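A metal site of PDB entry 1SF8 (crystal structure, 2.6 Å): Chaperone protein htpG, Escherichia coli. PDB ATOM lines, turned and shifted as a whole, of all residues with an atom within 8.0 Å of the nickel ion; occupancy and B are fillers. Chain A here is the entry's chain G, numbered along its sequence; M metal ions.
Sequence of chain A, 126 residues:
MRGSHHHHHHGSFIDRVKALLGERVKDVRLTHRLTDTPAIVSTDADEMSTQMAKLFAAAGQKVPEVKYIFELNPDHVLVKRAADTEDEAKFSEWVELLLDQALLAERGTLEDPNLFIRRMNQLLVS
Of the 12 residues printed, 4 come within 4 Å of the nickel ion.
The nearest printed residue that does not touch the nickel ion is Pro 74 (4.4 Å).
The nickel ion is bound by OD1 of Asp 75, 1.9 Å away.
NE2 of His 32 binds the nickel ion (2.0 Å).
ND1 of His 7 is bound to the nickel ion.
The nickel ion is bound by a ring nitrogen (NE2) of His 9, at 2.1 Å.
OD1 of Asn 73 sits close to N of Asp 75, at 3.2 Å.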
ATOM      1  N   HIS A   6      29.752  24.377  23.700  1.00  0.00           N
ATOM      2  CA  HIS A   6      30.305  25.554  22.979  1.00  0.00           C
ATOM      3  C   HIS A   6      29.301  26.028  21.930  1.00  0.00           C
ATOM      4  O   HIS A   6      29.689  26.524  20.864  1.00  0.00           O
ATOM      5  CB  HIS A   6      31.627  25.180  22.308  1.00  0.00           C
ATOM      6  N   HIS A   7      28.017  25.880  22.244  1.00  0.00           N
ATOM      7  CA  HIS A   7      26.937  26.260  21.327  1.00  0.00           C
ATOM      8  C   HIS A   7      26.130  27.483  21.743  1.00  0.00           C
ATOM      9  O   HIS A   7      24.917  27.534  21.502  1.00  0.00           O
ATOM     10  CB  HIS A   7      25.981  25.083  21.145  1.00  0.00           C
ATOM     11  CG  HIS A   7      26.430  24.087  20.135  1.00  0.00           C
ATOM     12  ND1 HIS A   7      26.221  24.250  18.781  1.00  0.00           N
ATOM     13  CD2 HIS A   7      27.058  22.890  20.279  1.00  0.00           C
ATOM     14  CE1 HIS A   7      26.706  23.202  18.134  1.00  0.00           C
ATOM     15  NE2 HIS A   7      27.219  22.367  19.024  1.00  0.00           N
ATOM     16  N   HIS A   8      26.761  28.453  22.370  1.00  0.00           N
ATOM     17  CA  HIS A   8      26.045  29.660  22.781  1.00  0.00           C
ATOM     18  C   HIS A   8      25.841  30.528  21.540  1.00  0.00           C
ATOM     19  O   HIS A   8      26.771  31.203  21.108  1.00  0.00           O
ATOM     20  CB  HIS A   8      26.843  30.417  23.845  1.00  0.00           C
ATOM     21  CG  HIS A   8      28.299  30.035  23.881  1.00  0.00           C
ATOM     22  ND1 HIS A   8      28.997  29.687  22.757  1.00  0.00           N
ATOM     23  CD2 HIS A   8      29.174  29.963  24.916  1.00  0.00           C
ATOM     24  CE1 HIS A   8      30.257  29.409  23.086  1.00  0.00           C
ATOM     25  NE2 HIS A   8      30.380  29.576  24.387  1.00  0.00           N
ATOM     26  N   HIS A   9      24.660  30.531  20.957  1.00  0.00           N
ATOM     27  CA  HIS A   9      24.429  31.330  19.771  1.00  0.00           C
ATOM     28  C   HIS A   9      23.956  32.745  20.131  1.00  0.00           C
ATOM     29  O   HIS A   9      22.959  32.907  20.838  1.00  0.00           O
ATOM     30  CB  HIS A   9      23.416  30.634  18.845  1.00  0.00           C
ATOM     31  CG  HIS A   9      23.807  29.239  18.454  1.00  0.00           C
ATOM     32  ND1 HIS A   9      24.880  28.968  17.638  1.00  0.00           N
ATOM     33  CD2 HIS A   9      23.306  28.035  18.820  1.00  0.00           C
ATOM     34  CE1 HIS A   9      25.023  27.663  17.514  1.00  0.00           C
ATOM     35  NE2 HIS A   9      24.075  27.077  18.212  1.00  0.00           N
ATOM     36  N   THR A  31      16.248  26.497  16.886  1.00  0.00           N
ATOM     37  CA  THR A  31      16.345  25.205  17.580  1.00  0.00           C
ATOM     38  C   THR A  31      17.247  24.280  16.784  1.00  0.00           C
ATOM     39  O   THR A  31      17.285  24.360  15.568  1.00  0.00           O
ATOM     40  CB  THR A  31      14.964  24.542  17.776  1.00  0.00           C
ATOM     41  OG1 THR A  31      14.536  23.975  16.538  1.00  0.00           O
ATOM     42  CG2 THR A  31      13.930  25.541  18.246  1.00  0.00           C
ATOM     43  N   HIS A  32      18.019  23.446  17.457  1.00  0.00           N
ATOM     44  CA  HIS A  32      18.909  22.526  16.760  1.00  0.00           C
ATOM     45  C   HIS A  32      18.129  21.368  16.155  1.00  0.00           C
ATOM     46  O   HIS A  32      16.983  21.101  16.536  1.00  0.00           O
ATOM     47  CB  HIS A  32      19.997  22.009  17.718  1.00  0.00           C
ATOM     48  CG  HIS A  32      20.986  23.053  18.119  1.00  0.00           C
ATOM     49  ND1 HIS A  32      20.641  24.120  18.923  1.00  0.00           N
ATOM     50  CD2 HIS A  32      22.269  23.257  17.750  1.00  0.00           C
ATOM     51  CE1 HIS A  32      21.672  24.938  19.016  1.00  0.00           C
ATOM     52  NE2 HIS A  32      22.666  24.448  18.316  1.00  0.00           N
ATOM     53  N   ARG A  33      18.754  20.682  15.202  1.00  0.00           N
ATOM     54  CA  ARG A  33      18.121  19.569  14.521  1.00  0.00           C
ATOM     55  C   ARG A  33      19.001  18.335  14.586  1.00  0.00           C
ATOM     56  O   ARG A  33      20.188  18.442  14.861  1.00  0.00           O
ATOM     57  CB  ARG A  33      17.892  19.929  13.042  1.00  0.00           C
ATOM     58  CG  ARG A  33      16.910  21.034  12.799  1.00  0.00           C
ATOM     59  CD  ARG A  33      15.506  20.502  12.609  1.00  0.00           C
ATOM     60  NE  ARG A  33      14.563  21.146  13.524  1.00  0.00           N
ATOM     61  CZ  ARG A  33      14.202  20.624  14.681  1.00  0.00           C
ATOM     62  NH1 ARG A  33      14.711  19.447  15.034  1.00  0.00           N
ATOM     63  NH2 ARG A  33      13.329  21.247  15.466  1.00  0.00           N
ATOM     64  N   ASN A  73      17.831  26.357  12.038  1.00  0.00           N
ATOM     65  CA  ASN A  73      18.923  25.571  12.593  1.00  0.00           C
ATOM     66  C   ASN A  73      20.245  26.319  12.741  1.00  0.00           C
ATOM     67  O   ASN A  73      21.053  26.384  11.805  1.00  0.00           O
ATOM     68  CB  ASN A  73      19.144  24.305  11.763  1.00  0.00           C
ATOM     69  CG  ASN A  73      20.264  23.458  12.313  1.00  0.00           C
ATOM     70  OD1 ASN A  73      20.758  23.703  13.407  1.00  0.00           O
ATOM     71  ND2 ASN A  73      20.680  22.445  11.559  1.00  0.00           N
ATOM     72  N   PRO A  74      20.511  26.848  13.934  1.00  0.00           N
ATOM     73  CA  PRO A  74      21.710  27.608  14.295  1.00  0.00           C
ATOM     74  C   PRO A  74      23.033  27.033  13.822  1.00  0.00           C
ATOM     75  O   PRO A  74      23.969  27.792  13.565  1.00  0.00           O
ATOM     76  CB  PRO A  74      21.662  27.631  15.814  1.00  0.00           C
ATOM     77  CG  PRO A  74      20.235  27.583  16.114  1.00  0.00           C
ATOM     78  CD  PRO A  74      19.727  26.549  15.141  1.00  0.00           C
ATOM     79  N   ASP A  75      23.176  25.721  13.733  1.00  0.00           N
ATOM     80  CA  ASP A  75      24.478  25.237  13.329  1.00  0.00           C
ATOM     81  C   ASP A  75      24.639  25.123  11.817  1.00  0.00           C
ATOM     82  O   ASP A  75      25.736  24.876  11.338  1.00  0.00           O
ATOM     83  CB  ASP A  75      24.808  23.863  13.955  1.00  0.00           C
ATOM     84  CG  ASP A  75      24.805  23.860  15.484  1.00  0.00           C
ATOM     85  OD1 ASP A  75      24.966  24.902  16.153  1.00  0.00           O
ATOM     86  OD2 ASP A  75      24.639  22.762  16.036  1.00  0.00           O
ATOM     87  N   HIS A  76      23.566  25.296  11.066  1.00  0.00           N
ATOM     88  CA  HIS A  76      23.681  25.165   9.626  1.00  0.00           C
ATOM     89  C   HIS A  76      24.370  26.330   8.899  1.00  0.00           C
ATOM     90  O   HIS A  76      24.006  27.502   9.074  1.00  0.00           O
ATOM     91  CB  HIS A  76      22.318  24.943   8.988  1.00  0.00           C
ATOM     92  CG  HIS A  76      22.391  24.392   7.600  1.00  0.00           C
ATOM     93  ND1 HIS A  76      22.284  23.039   7.335  1.00  0.00           N
ATOM     94  CD2 HIS A  76      22.679  24.978   6.414  1.00  0.00           C
ATOM     95  CE1 HIS A  76      22.504  22.824   6.057  1.00  0.00           C
ATOM     96  NE2 HIS A  76      22.753  23.990   5.469  1.00  0.00           N
ATOM     97  N   LYS A  80      23.751  30.451   9.020  1.00  0.00           N
ATOM     98  CA  LYS A  80      24.758  31.345   9.541  1.00  0.00           C
ATOM     99  C   LYS A  80      25.053  32.411   8.519  1.00  0.00           C
ATOM    100  O   LYS A  80      25.176  33.593   8.835  1.00  0.00           O
ATOM    101  CB  LYS A  80      26.028  30.571   9.882  1.00  0.00           C
ATOM    102  CG  LYS A  80      25.964  29.941  11.262  1.00  0.00           C
ATOM    103  CD  LYS A  80      27.076  28.929  11.493  1.00  0.00           C
ATOM    104  CE  LYS A  80      27.013  28.393  12.923  1.00  0.00           C
ATOM    105  NZ  LYS A  80      28.041  27.360  13.183  1.00  0.00           N
HETATM  106 NI    NI M   1      24.508  25.038  17.970  1.00  0.00          NI
